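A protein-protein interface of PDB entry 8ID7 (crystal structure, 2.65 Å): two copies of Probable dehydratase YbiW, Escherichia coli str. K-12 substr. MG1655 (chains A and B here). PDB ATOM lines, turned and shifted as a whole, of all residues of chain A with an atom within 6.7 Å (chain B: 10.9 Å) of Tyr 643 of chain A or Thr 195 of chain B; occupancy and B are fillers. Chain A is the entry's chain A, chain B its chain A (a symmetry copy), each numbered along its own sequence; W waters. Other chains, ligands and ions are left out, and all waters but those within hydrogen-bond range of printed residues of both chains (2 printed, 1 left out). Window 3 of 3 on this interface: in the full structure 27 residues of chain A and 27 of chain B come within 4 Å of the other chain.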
ATOM      1  N   ARG A 509      18.164   3.950  40.489  1.00  0.00           N
ATOM      2  CA  ARG A 509      18.230   3.781  39.040  1.00  0.00           C
ATOM      3  C   ARG A 509      16.904   4.142  38.381  1.00  0.00           C
ATOM      4  O   ARG A 509      16.885   4.525  37.207  1.00  0.00           O
ATOM      5  CB  ARG A 509      18.653   2.354  38.663  1.00  0.00           C
ATOM      6  CG  ARG A 509      20.186   2.079  38.712  1.00  0.00           C
ATOM      7  CD  ARG A 509      20.549   0.673  38.149  1.00  0.00           C
ATOM      8  NE  ARG A 509      21.852   0.169  38.594  1.00  0.00           N
ATOM      9  CZ  ARG A 509      22.038  -0.974  39.267  1.00  0.00           C
ATOM     10  NH1 ARG A 509      20.995  -1.755  39.566  1.00  0.00           N
ATOM     11  NH2 ARG A 509      23.269  -1.348  39.646  1.00  0.00           N
ATOM     12  N   THR A 512      16.345   8.195  38.577  1.00  0.00           N
ATOM     13  CA  THR A 512      17.188   8.885  37.610  1.00  0.00           C
ATOM     14  C   THR A 512      16.574   8.846  36.208  1.00  0.00           C
ATOM     15  O   THR A 512      16.543   9.862  35.507  1.00  0.00           O
ATOM     16  CB  THR A 512      18.584   8.271  37.619  1.00  0.00           C
ATOM     17  OG1 THR A 512      19.109   8.371  38.933  1.00  0.00           O
ATOM     18  CG2 THR A 512      19.506   9.005  36.686  1.00  0.00           C
ATOM     19  N   ARG A 513      16.082   7.683  35.779  1.00  0.00           N
ATOM     20  CA  ARG A 513      15.372   7.616  34.511  1.00  0.00           C
ATOM     21  C   ARG A 513      14.256   8.650  34.481  1.00  0.00           C
ATOM     22  O   ARG A 513      14.193   9.504  33.590  1.00  0.00           O
ATOM     23  CB  ARG A 513      14.820   6.202  34.291  1.00  0.00           C
ATOM     24  CG  ARG A 513      14.074   5.992  32.975  1.00  0.00           C
ATOM     25  CD  ARG A 513      13.670   4.555  32.795  1.00  0.00           C
ATOM     26  NE  ARG A 513      14.831   3.669  32.741  1.00  0.00           N
ATOM     27  CZ  ARG A 513      15.633   3.539  31.679  1.00  0.00           C
ATOM     28  NH1 ARG A 513      15.395   4.252  30.570  1.00  0.00           N
ATOM     29  NH2 ARG A 513      16.677   2.699  31.718  1.00  0.00           N
ATOM     30  N   LYS A 514      13.378   8.600  35.472  1.00  0.00           N
ATOM     31  CA  LYS A 514      12.294   9.565  35.533  1.00  0.00           C
ATOM     32  C   LYS A 514      12.817  11.002  35.420  1.00  0.00           C
ATOM     33  O   LYS A 514      12.319  11.804  34.615  1.00  0.00           O
ATOM     34  CB  LYS A 514      11.508   9.341  36.826  1.00  0.00           C
ATOM     35  CG  LYS A 514      10.810   7.984  36.850  1.00  0.00           C
ATOM     36  CD  LYS A 514       9.753   7.864  35.739  1.00  0.00           C
ATOM     37  CE  LYS A 514       9.962   6.614  34.910  1.00  0.00           C
ATOM     38  NZ  LYS A 514       8.667   6.118  34.405  1.00  0.00           N
ATOM     39  N   ILE A 516      15.340  12.137  34.020  1.00  0.00           N
ATOM     40  CA  ILE A 516      15.776  12.437  32.661  1.00  0.00           C
ATOM     41  C   ILE A 516      14.574  12.542  31.716  1.00  0.00           C
ATOM     42  O   ILE A 516      14.524  13.419  30.847  1.00  0.00           O
ATOM     43  CB  ILE A 516      16.789  11.382  32.199  1.00  0.00           C
ATOM     44  CG1 ILE A 516      17.988  11.385  33.134  1.00  0.00           C
ATOM     45  CG2 ILE A 516      17.229  11.653  30.777  1.00  0.00           C
ATOM     46  CD1 ILE A 516      18.767  12.666  33.088  1.00  0.00           C
ATOM     47  N   GLU A 517      13.585  11.662  31.876  1.00  0.00           N
ATOM     48  CA  GLU A 517      12.351  11.803  31.117  1.00  0.00           C
ATOM     49  C   GLU A 517      11.707  13.163  31.379  1.00  0.00           C
ATOM     50  O   GLU A 517      11.239  13.831  30.449  1.00  0.00           O
ATOM     51  CB  GLU A 517      11.387  10.664  31.465  1.00  0.00           C
ATOM     52  CG  GLU A 517      11.900   9.267  31.103  1.00  0.00           C
ATOM     53  CD  GLU A 517      10.905   8.146  31.423  1.00  0.00           C
ATOM     54  OE1 GLU A 517       9.819   8.413  31.988  1.00  0.00           O
ATOM     55  OE2 GLU A 517      11.220   6.983  31.094  1.00  0.00           O
ATOM     56  N   ILE A 518      11.662  13.587  32.650  1.00  0.00           N
ATOM     57  CA  ILE A 518      11.108  14.905  32.964  1.00  0.00           C
ATOM     58  C   ILE A 518      11.945  15.989  32.296  1.00  0.00           C
ATOM     59  O   ILE A 518      11.423  16.924  31.666  1.00  0.00           O
ATOM     60  CB  ILE A 518      11.038  15.120  34.490  1.00  0.00           C
ATOM     61  CG1 ILE A 518      10.110  14.088  35.171  1.00  0.00           C
ATOM     62  CG2 ILE A 518      10.658  16.586  34.828  1.00  0.00           C
ATOM     63  CD1 ILE A 518       9.687  14.463  36.611  1.00  0.00           C
ATOM     64  N   TYR A 520      13.650  15.854  29.754  1.00  0.00           N
ATOM     65  CA  TYR A 520      13.529  15.860  28.300  1.00  0.00           C
ATOM     66  C   TYR A 520      12.325  16.672  27.870  1.00  0.00           C
ATOM     67  O   TYR A 520      12.393  17.409  26.884  1.00  0.00           O
ATOM     68  CB  TYR A 520      13.472  14.430  27.757  1.00  0.00           C
ATOM     69  CG  TYR A 520      14.746  14.038  27.041  1.00  0.00           C
ATOM     70  CD1 TYR A 520      15.896  13.685  27.743  1.00  0.00           C
ATOM     71  CD2 TYR A 520      14.814  14.069  25.657  1.00  0.00           C
ATOM     72  CE1 TYR A 520      17.064  13.349  27.079  1.00  0.00           C
ATOM     73  CE2 TYR A 520      15.972  13.733  24.987  1.00  0.00           C
ATOM     74  CZ  TYR A 520      17.093  13.373  25.699  1.00  0.00           C
ATOM     75  OH  TYR A 520      18.217  13.044  24.994  1.00  0.00           O
ATOM     76  N   ASP A 638      26.851   6.166  37.706  1.00  0.00           N
ATOM     77  CA  ASP A 638      26.876   5.100  36.722  1.00  0.00           C
ATOM     78  C   ASP A 638      25.615   5.094  35.864  1.00  0.00           C
ATOM     79  O   ASP A 638      25.659   4.613  34.722  1.00  0.00           O
ATOM     80  CB  ASP A 638      27.068   3.752  37.419  1.00  0.00           C
ATOM     81  CG  ASP A 638      28.540   3.449  37.753  1.00  0.00           C
ATOM     82  OD1 ASP A 638      29.428   4.299  37.504  1.00  0.00           O
ATOM     83  OD2 ASP A 638      28.804   2.342  38.275  1.00  0.00           O
ATOM     84  N   GLU A 639      24.504   5.633  36.374  1.00  0.00           N
ATOM     85  CA  GLU A 639      23.276   5.690  35.586  1.00  0.00           C
ATOM     86  C   GLU A 639      23.386   6.731  34.493  1.00  0.00           C
ATOM     87  O   GLU A 639      23.021   6.477  33.344  1.00  0.00           O
ATOM     88  CB  GLU A 639      22.078   6.009  36.473  1.00  0.00           C
ATOM     89  CG  GLU A 639      21.449   4.824  37.137  1.00  0.00           C
ATOM     90  CD  GLU A 639      20.948   3.807  36.145  1.00  0.00           C
ATOM     91  OE1 GLU A 639      20.011   4.123  35.377  1.00  0.00           O
ATOM     92  OE2 GLU A 639      21.502   2.684  36.134  1.00  0.00           O
ATOM     93  N   LEU A 640      23.875   7.917  34.838  1.00  0.00           N
ATOM     94  CA  LEU A 640      23.897   9.010  33.883  1.00  0.00           C
ATOM     95  C   LEU A 640      24.608   8.619  32.597  1.00  0.00           C
ATOM     96  O   LEU A 640      24.411   9.273  31.567  1.00  0.00           O
ATOM     97  CB  LEU A 640      24.557  10.236  34.520  1.00  0.00           C
ATOM     98  CG  LEU A 640      23.844  10.743  35.771  1.00  0.00           C
ATOM     99  CD1 LEU A 640      24.542  11.992  36.323  1.00  0.00           C
ATOM    100  CD2 LEU A 640      22.405  11.038  35.470  1.00  0.00           C
ATOM    101  N   LYS A 641      25.405   7.546  32.624  1.00  0.00           N
ATOM    102  CA  LYS A 641      26.255   7.212  31.491  1.00  0.00           C
ATOM    103  C   LYS A 641      25.479   6.635  30.316  1.00  0.00           C
ATOM    104  O   LYS A 641      25.976   6.673  29.186  1.00  0.00           O
ATOM    105  CB  LYS A 641      27.329   6.219  31.916  1.00  0.00           C
ATOM    106  CG  LYS A 641      28.594   6.844  32.453  1.00  0.00           C
ATOM    107  CD  LYS A 641      29.354   5.838  33.309  1.00  0.00           C
ATOM    108  CE  LYS A 641      30.180   6.527  34.407  1.00  0.00           C
ATOM    109  NZ  LYS A 641      30.901   5.548  35.307  1.00  0.00           N
ATOM    110  N   GLN A 642      24.283   6.103  30.541  1.00  0.00           N
ATOM    111  CA  GLN A 642      23.509   5.505  29.460  1.00  0.00           C
ATOM    112  C   GLN A 642      22.464   6.456  28.899  1.00  0.00           C
ATOM    113  O   GLN A 642      21.541   6.019  28.197  1.00  0.00           O
ATOM    114  CB  GLN A 642      22.846   4.223  29.942  1.00  0.00           C
ATOM    115  CG  GLN A 642      21.618   4.488  30.757  1.00  0.00           C
ATOM    116  CD  GLN A 642      20.960   3.207  31.200  1.00  0.00           C
ATOM    117  OE1 GLN A 642      20.693   2.320  30.380  1.00  0.00           O
ATOM    118  NE2 GLN A 642      20.704   3.089  32.509  1.00  0.00           N
ATOM    119  N   TYR A 643      22.595   7.742  29.198  1.00  0.00           N
ATOM    120  CA  TYR A 643      21.745   8.797  28.687  1.00  0.00           C
ATOM    121  C   TYR A 643      22.599   9.821  27.933  1.00  0.00           C
ATOM    122  O   TYR A 643      23.835   9.828  28.018  1.00  0.00           O
ATOM    123  CB  TYR A 643      20.961   9.444  29.832  1.00  0.00           C
ATOM    124  CG  TYR A 643      20.147   8.445  30.627  1.00  0.00           C
ATOM    125  CD1 TYR A 643      18.909   8.004  30.178  1.00  0.00           C
ATOM    126  CD2 TYR A 643      20.621   7.927  31.828  1.00  0.00           C
ATOM    127  CE1 TYR A 643      18.166   7.079  30.909  1.00  0.00           C
ATOM    128  CE2 TYR A 643      19.888   6.999  32.559  1.00  0.00           C
ATOM    129  CZ  TYR A 643      18.665   6.581  32.099  1.00  0.00           C
ATOM    130  OH  TYR A 643      17.941   5.667  32.829  1.00  0.00           O
ATOM    131  N   HIS A 644      21.919  10.655  27.142  1.00  0.00           N
ATOM    132  CA  HIS A 644      22.495  11.799  26.444  1.00  0.00           C
ATOM    133  C   HIS A 644      21.483  12.927  26.549  1.00  0.00           C
ATOM    134  O   HIS A 644      20.281  12.680  26.488  1.00  0.00           O
ATOM    135  CB  HIS A 644      22.788  11.532  24.950  1.00  0.00           C
ATOM    136  CG  HIS A 644      23.603  10.307  24.682  1.00  0.00           C
ATOM    137  ND1 HIS A 644      24.806  10.059  25.302  1.00  0.00           N
ATOM    138  CD2 HIS A 644      23.396   9.271  23.836  1.00  0.00           C
ATOM    139  CE1 HIS A 644      25.296   8.912  24.865  1.00  0.00           C
ATOM    140  NE2 HIS A 644      24.457   8.412  23.978  1.00  0.00           N
ATOM    141  N   ASN A 645      21.949  14.157  26.700  1.00  0.00           N
ATOM    142  CA  ASN A 645      21.006  15.253  26.868  1.00  0.00           C
ATOM    143  C   ASN A 645      20.439  15.634  25.500  1.00  0.00           C
ATOM    144  O   ASN A 645      20.904  15.156  24.466  1.00  0.00           O
ATOM    145  CB  ASN A 645      21.674  16.417  27.622  1.00  0.00           C
ATOM    146  CG  ASN A 645      22.508  17.328  26.726  1.00  0.00           C
ATOM    147  OD1 ASN A 645      21.969  18.048  25.864  1.00  0.00           O
ATOM    148  ND2 ASN A 645      23.816  17.339  26.957  1.00  0.00           N
ATOM    149  N   PRO A 646      19.370  16.435  25.473  1.00  0.00           N
ATOM    150  CA  PRO A 646      18.667  16.697  24.204  1.00  0.00           C
ATOM    151  C   PRO A 646      19.524  17.246  23.077  1.00  0.00           C
ATOM    152  O   PRO A 646      19.152  17.086  21.910  1.00  0.00           O
ATOM    153  CB  PRO A 646      17.596  17.697  24.628  1.00  0.00           C
ATOM    154  CG  PRO A 646      17.233  17.224  26.015  1.00  0.00           C
ATOM    155  CD  PRO A 646      18.534  16.786  26.635  1.00  0.00           C
ATOM    156  N   TYR A 648      22.402  16.093  22.218  1.00  0.00           N
ATOM    157  CA  TYR A 648      23.282  15.063  21.691  1.00  0.00           C
ATOM    158  C   TYR A 648      23.080  14.944  20.193  1.00  0.00           C
ATOM    159  O   TYR A 648      21.953  14.792  19.719  1.00  0.00           O
ATOM    160  CB  TYR A 648      23.013  13.718  22.377  1.00  0.00           C
ATOM    161  CG  TYR A 648      24.013  12.648  22.011  1.00  0.00           C
ATOM    162  CD1 TYR A 648      25.128  12.387  22.806  1.00  0.00           C
ATOM    163  CD2 TYR A 648      23.859  11.902  20.849  1.00  0.00           C
ATOM    164  CE1 TYR A 648      26.049  11.396  22.451  1.00  0.00           C
ATOM    165  CE2 TYR A 648      24.773  10.916  20.488  1.00  0.00           C
ATOM    166  CZ  TYR A 648      25.867  10.671  21.285  1.00  0.00           C
ATOM    167  OH  TYR A 648      26.745   9.682  20.898  1.00  0.00           O
ATOM    168  N   GLY A 655      27.548  16.512  24.787  1.00  0.00           N
ATOM    169  CA  GLY A 655      26.109  16.274  24.856  1.00  0.00           C
ATOM    170  C   GLY A 655      25.630  15.347  25.954  1.00  0.00           C
ATOM    171  O   GLY A 655      24.640  14.643  25.753  1.00  0.00           O
ATOM    172  N   ASN A 656      26.277  15.352  27.124  1.00  0.00           N
ATOM    173  CA  ASN A 656      26.047  14.341  28.159  1.00  0.00           C
ATOM    174  C   ASN A 656      25.713  15.001  29.506  1.00  0.00           C
ATOM    175  O   ASN A 656      25.560  16.223  29.607  1.00  0.00           O
ATOM    176  CB  ASN A 656      27.268  13.412  28.293  1.00  0.00           C
ATOM    177  CG  ASN A 656      27.402  12.435  27.113  1.00  0.00           C
ATOM    178  OD1 ASN A 656      26.467  11.692  26.785  1.00  0.00           O
ATOM    179  ND2 ASN A 656      28.571  12.438  26.469  1.00  0.00           N
ATOM    180  N   TYR A 657      25.594  14.174  30.551  1.00  0.00           N
ATOM    181  CA  TYR A 657      25.327  14.604  31.918  1.00  0.00           C
ATOM    182  C   TYR A 657      26.521  14.330  32.831  1.00  0.00           C
ATOM    183  O   TYR A 657      27.434  13.562  32.499  1.00  0.00           O
ATOM    184  CB  TYR A 657      24.106  13.883  32.491  1.00  0.00           C
ATOM    185  CG  TYR A 657      22.833  14.117  31.725  1.00  0.00           C
ATOM    186  CD1 TYR A 657      22.105  15.288  31.892  1.00  0.00           C
ATOM    187  CD2 TYR A 657      22.343  13.151  30.838  1.00  0.00           C
ATOM    188  CE1 TYR A 657      20.931  15.499  31.191  1.00  0.00           C
ATOM    189  CE2 TYR A 657      21.155  13.347  30.138  1.00  0.00           C
ATOM    190  CZ  TYR A 657      20.462  14.523  30.315  1.00  0.00           C
ATOM    191  OH  TYR A 657      19.308  14.745  29.626  1.00  0.00           O
ATOM    192  N   ARG B 191       7.779   0.420  21.634  1.00  0.00           N
ATOM    193  CA  ARG B 191       9.190   0.530  21.319  1.00  0.00           C
ATOM    194  C   ARG B 191       9.703   1.949  21.498  1.00  0.00           C
ATOM    195  O   ARG B 191      10.831   2.248  21.085  1.00  0.00           O
ATOM    196  CB  ARG B 191       9.454   0.058  19.879  1.00  0.00           C
ATOM    197  CG  ARG B 191       9.330  -1.455  19.655  1.00  0.00           C
ATOM    198  CD  ARG B 191       9.667  -1.891  18.224  1.00  0.00           C
ATOM    199  NE  ARG B 191       8.549  -1.734  17.286  1.00  0.00           N
ATOM    200  CZ  ARG B 191       8.600  -1.045  16.140  1.00  0.00           C
ATOM    201  NH1 ARG B 191       9.712  -0.423  15.762  1.00  0.00           N
ATOM    202  NH2 ARG B 191       7.524  -0.968  15.367  1.00  0.00           N
ATOM    203  N   ILE B 192       8.895   2.825  22.091  1.00  0.00           N
ATOM    204  CA  ILE B 192       9.257   4.223  22.304  1.00  0.00           C
ATOM    205  C   ILE B 192      10.166   4.312  23.526  1.00  0.00           C
ATOM    206  O   ILE B 192       9.972   3.592  24.513  1.00  0.00           O
ATOM    207  CB  ILE B 192       7.968   5.063  22.460  1.00  0.00           C
ATOM    208  CG1 ILE B 192       7.321   5.299  21.091  1.00  0.00           C
ATOM    209  CG2 ILE B 192       8.210   6.396  23.159  1.00  0.00           C
ATOM    210  CD1 ILE B 192       8.140   6.219  20.157  1.00  0.00           C
ATOM    211  N   ASN B 193      11.184   5.165  23.464  1.00  0.00           N
ATOM    212  CA  ASN B 193      12.057   5.440  24.605  1.00  0.00           C
ATOM    213  C   ASN B 193      11.994   6.924  24.907  1.00  0.00           C
ATOM    214  O   ASN B 193      12.388   7.742  24.072  1.00  0.00           O
ATOM    215  CB  ASN B 193      13.504   5.040  24.322  1.00  0.00           C
ATOM    216  CG  ASN B 193      14.439   5.321  25.503  1.00  0.00           C
ATOM    217  OD1 ASN B 193      14.010   5.807  26.553  1.00  0.00           O
ATOM    218  ND2 ASN B 193      15.725   4.999  25.336  1.00  0.00           N
ATOM    219  N   LEU B 194      11.539   7.275  26.102  1.00  0.00           N
ATOM    220  CA  LEU B 194      11.296   8.677  26.402  1.00  0.00           C
ATOM    221  C   LEU B 194      12.546   9.461  26.807  1.00  0.00           C
ATOM    222  O   LEU B 194      12.398  10.613  27.226  1.00  0.00           O
ATOM    223  CB  LEU B 194      10.235   8.786  27.491  1.00  0.00           C
ATOM    224  CG  LEU B 194       8.860   8.440  26.927  1.00  0.00           C
ATOM    225  CD1 LEU B 194       7.838   8.396  28.024  1.00  0.00           C
ATOM    226  CD2 LEU B 194       8.439   9.406  25.820  1.00  0.00           C
ATOM    227  N   THR B 195      13.759   8.902  26.724  1.00  0.00           N
ATOM    228  CA  THR B 195      14.967   9.708  26.912  1.00  0.00           C
ATOM    229  C   THR B 195      15.711   9.905  25.597  1.00  0.00           C
ATOM    230  O   THR B 195      16.892  10.262  25.597  1.00  0.00           O
ATOM    231  CB  THR B 195      15.911   9.122  27.979  1.00  0.00           C
ATOM    232  OG1 THR B 195      16.414   7.836  27.572  1.00  0.00           O
ATOM    233  CG2 THR B 195      15.220   9.024  29.335  1.00  0.00           C
ATOM    234  N   VAL B 196      15.019   9.695  24.483  1.00  0.00           N
ATOM    235  CA  VAL B 196      15.554   9.827  23.135  1.00  0.00           C
ATOM    236  C   VAL B 196      14.749  10.917  22.443  1.00  0.00           C
ATOM    237  O   VAL B 196      13.533  10.770  22.261  1.00  0.00           O
ATOM    238  CB  VAL B 196      15.453   8.498  22.372  1.00  0.00           C
ATOM    239  CG1 VAL B 196      16.003   8.615  20.958  1.00  0.00           C
ATOM    240  CG2 VAL B 196      16.130   7.380  23.173  1.00  0.00           C
ATOM    241  N   LEU B 197      15.411  12.008  22.064  1.00  0.00           N
ATOM    242  CA  LEU B 197      14.668  13.161  21.577  1.00  0.00           C
ATOM    243  C   LEU B 197      13.618  12.729  20.566  1.00  0.00           C
ATOM    244  O   LEU B 197      12.422  12.958  20.758  1.00  0.00           O
ATOM    245  CB  LEU B 197      15.626  14.179  20.971  1.00  0.00           C
ATOM    246  CG  LEU B 197      15.046  15.544  20.575  1.00  0.00           C
ATOM    247  CD1 LEU B 197      14.310  16.224  21.726  1.00  0.00           C
ATOM    248  CD2 LEU B 197      16.166  16.444  20.065  1.00  0.00           C
ATOM    249  N   GLU B 198      14.055  12.050  19.495  1.00  0.00           N
ATOM    250  CA  GLU B 198      13.150  11.711  18.400  1.00  0.00           C
ATOM    251  C   GLU B 198      11.970  10.865  18.874  1.00  0.00           C
ATOM    252  O   GLU B 198      10.865  10.974  18.319  1.00  0.00           O
ATOM    253  CB  GLU B 198      13.916  10.981  17.301  1.00  0.00           C
ATOM    254  CG  GLU B 198      14.766  11.903  16.444  1.00  0.00           C
ATOM    255  CD  GLU B 198      15.287  11.222  15.182  1.00  0.00           C
ATOM    256  OE1 GLU B 198      15.451   9.978  15.197  1.00  0.00           O
ATOM    257  OE2 GLU B 198      15.523  11.932  14.175  1.00  0.00           O
ATOM    258  N   ASP B 199      12.185  10.018  19.898  1.00  0.00           N
ATOM    259  CA  ASP B 199      11.094   9.217  20.449  1.00  0.00           C
ATOM    260  C   ASP B 199      10.118  10.077  21.243  1.00  0.00           C
ATOM    261  O   ASP B 199       8.918   9.775  21.282  1.00  0.00           O
ATOM    262  CB  ASP B 199      11.649   8.078  21.319  1.00  0.00           C
ATOM    263  CG  ASP B 199      12.263   6.932  20.486  1.00  0.00           C
ATOM    264  OD1 ASP B 199      12.512   7.131  19.274  1.00  0.00           O
ATOM    265  OD2 ASP B 199      12.489   5.824  21.027  1.00  0.00           O
ATOM    266  N   LEU B 200      10.595  11.164  21.844  1.00  0.00           N
ATOM    267  CA  LEU B 200       9.703  12.011  22.625  1.00  0.00           C
ATOM    268  C   LEU B 200       8.646  12.654  21.744  1.00  0.00           C
ATOM    269  O   LEU B 200       7.478  12.747  22.139  1.00  0.00           O
ATOM    270  CB  LEU B 200      10.490  13.086  23.369  1.00  0.00           C
ATOM    271  CG  LEU B 200       9.525  13.972  24.135  1.00  0.00           C
ATOM    272  CD1 LEU B 200       8.951  13.152  25.273  1.00  0.00           C
ATOM    273  CD2 LEU B 200      10.159  15.249  24.652  1.00  0.00           C
ATOM    274  N   HIS B 201       9.044  13.134  20.560  1.00  0.00           N
ATOM    275  CA  HIS B 201       8.096  13.668  19.578  1.00  0.00           C
ATOM    276  C   HIS B 201       7.303  12.563  18.901  1.00  0.00           C
ATOM    277  O   HIS B 201       6.149  12.769  18.515  1.00  0.00           O
ATOM    278  CB  HIS B 201       8.829  14.435  18.490  1.00  0.00           C
ATOM    279  CG  HIS B 201       9.390  15.736  18.931  1.00  0.00           C
ATOM    280  ND1 HIS B 201      10.741  15.999  18.900  1.00  0.00           N
ATOM    281  CD2 HIS B 201       8.790  16.863  19.370  1.00  0.00           C
ATOM    282  CE1 HIS B 201      10.952  17.229  19.327  1.00  0.00           C
ATOM    283  NE2 HIS B 201       9.786  17.775  19.624  1.00  0.00           N
ATOM    284  N   GLY B 202       7.941  11.417  18.663  1.00  0.00           N
ATOM    285  CA  GLY B 202       7.247  10.308  18.040  1.00  0.00           C
ATOM    286  C   GLY B 202       6.032   9.848  18.819  1.00  0.00           C
ATOM    287  O   GLY B 202       5.047   9.395  18.223  1.00  0.00           O
ATOM    288  N   GLU B 203       6.079   9.948  20.156  1.00  0.00           N
ATOM    289  CA  GLU B 203       4.985   9.422  20.961  1.00  0.00           C
ATOM    290  C   GLU B 203       3.825  10.394  21.025  1.00  0.00           C
ATOM    291  O   GLU B 203       2.679   9.962  21.199  1.00  0.00           O
ATOM    292  CB  GLU B 203       5.461   9.064  22.378  1.00  0.00           C
ATOM    293  CG  GLU B 203       4.331   8.763  23.415  1.00  0.00           C
ATOM    294  CD  GLU B 203       3.549   7.456  23.173  1.00  0.00           C
ATOM    295  OE1 GLU B 203       3.729   6.816  22.106  1.00  0.00           O
ATOM    296  OE2 GLU B 203       2.728   7.082  24.050  1.00  0.00           O
HETATM  297  O   HOH W   1      10.431  12.285  28.272  1.00  0.00           O
HETATM  298  O   HOH W   2      18.634  12.555  22.345  1.00  0.00           O
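No residue of chain B comes within 4 Å of Thr 512 of chain A.
No residue of chain B comes within 4 Å of Arg 513 of chain A.
Ile 516 of chain A touches just one residue of chain B: Thr 195.
Printed residues of chain B within 4 Å of Tyr 520 of chain A: Thr 195 (3.1 Å), Val 196 (3.99 Å), Leu 197 (3.4 Å) and Leu 200 (3.8 Å).
No residue of chain B comes within 4 Å of Glu 639 of chain A.
Tyr 643 of chain A touches one residue of chain B.
His 644 of chain A touches none of the printed residues of chain B.
Of the printed residues of chain B, Pro 646 of chain A touches Leu 197 (3.6 Å).
No residue of chain B comes within 4 Å of Asn 656 of chain A.
Ile 192 of chain B touches none of the printed residues of chain A.
Thr 195 of chain B touches just these residues of chain A: Ile 516 (3.6 Å), Glu 517 (3.8 Å), Tyr 520 (3.1 Å) and Tyr 643 (3.6 Å).
Of the printed residues of chain A, Val 196 of chain B touches Tyr 520.
Printed residues of chain A within 4 Å of Leu 200 of chain B: Tyr 520.
The nearest residue of chain B that does not touch Tyr 643 of chain A is Asn 193 of chain B (6.2 Å).
The nearest residue of chain A that does not touch Thr 195 of chain B is His 644 of chain A (4.3 Å).
Of the 21 printed residues of chain A, 5 touch a printed residue of chain B.
Hydrophobic or aromatic side chains of chain A that line the printed part of chain B: Ile 516, Tyr 520 and Tyr 643.
Printed residues of chain B that touch a printed residue of chain A: Thr 195, Val 196, Leu 197 and Leu 200.
Among the printed residues, 8 pairs touch across the chains.
Among the printed residues, merely in contact across the chains: Tyr 520 of chain A with Leu 197 of chain B (3.4 Å), Pro 646 of chain A with Leu 197 of chain B (3.6 Å), Ile 516 of chain A with Thr 195 of chain B (3.6 Å), Tyr 643 of chain A with Thr 195 of chain B (3.6 Å), Glu 517 of chain A with Thr 195 of chain B (3.8 Å), Tyr 520 of chain A with Leu 200 of chain B (3.8 Å) and Tyr 520 of chain A with Val 196 of chain B (3.99 Å).
The backbone carbonyl oxygen (O) of Tyr 643 of chain A lies close to the side-chain amide oxygen (OD1) of Asn 656 of chain A, at 3.5 Å.
NH2 of Arg 513 of chain A sits close to OH of Tyr 643 of chain A, at 3.4 Å.
The side-chain carboxylate (OE1) of Glu 517 of chain A lies within salt-bridge range of the side-chain amino group (NZ) of Lys 514 of chain A, at 3.5 Å.
The side-chain hydroxyl (OH) of Tyr 520 of chain A lies close to the backbone carbonyl oxygen (O) of Asn 645 of chain A (3.5 Å).
The side-chain amide oxygen (OD1) of Asn 193 of chain B lies within hydrogen-bond range of the backbone NH (N) of Thr 195 of chain B, at 3.1 Å.
The backbone carbonyl oxygen of His 644 of chain A lies within hydrogen-bond range of the side-chain hydroxyl of Tyr 520 of chain A (2.6 Å).
O of Thr 195 of chain B sits close to OH of Tyr 520 of chain A, 3.1 Å away.
No position is printed for both chains.
Of the 8 pairs that touch across the chains among the printed residues, none has its exchanged pair printed and touching as well.
Water W2 bridges the side-chain hydroxyl (OH) of Tyr 520 of chain A (2.7 Å) and the backbone NH (N) of Leu 197 of chain B (3.3 Å).
Water W1 bridges the backbone carbonyl oxygen (O) of Leu 194 of chain B (2.8 Å) and the backbone carbonyl oxygen (O) of Glu 517 of chain A (2.8 Å).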
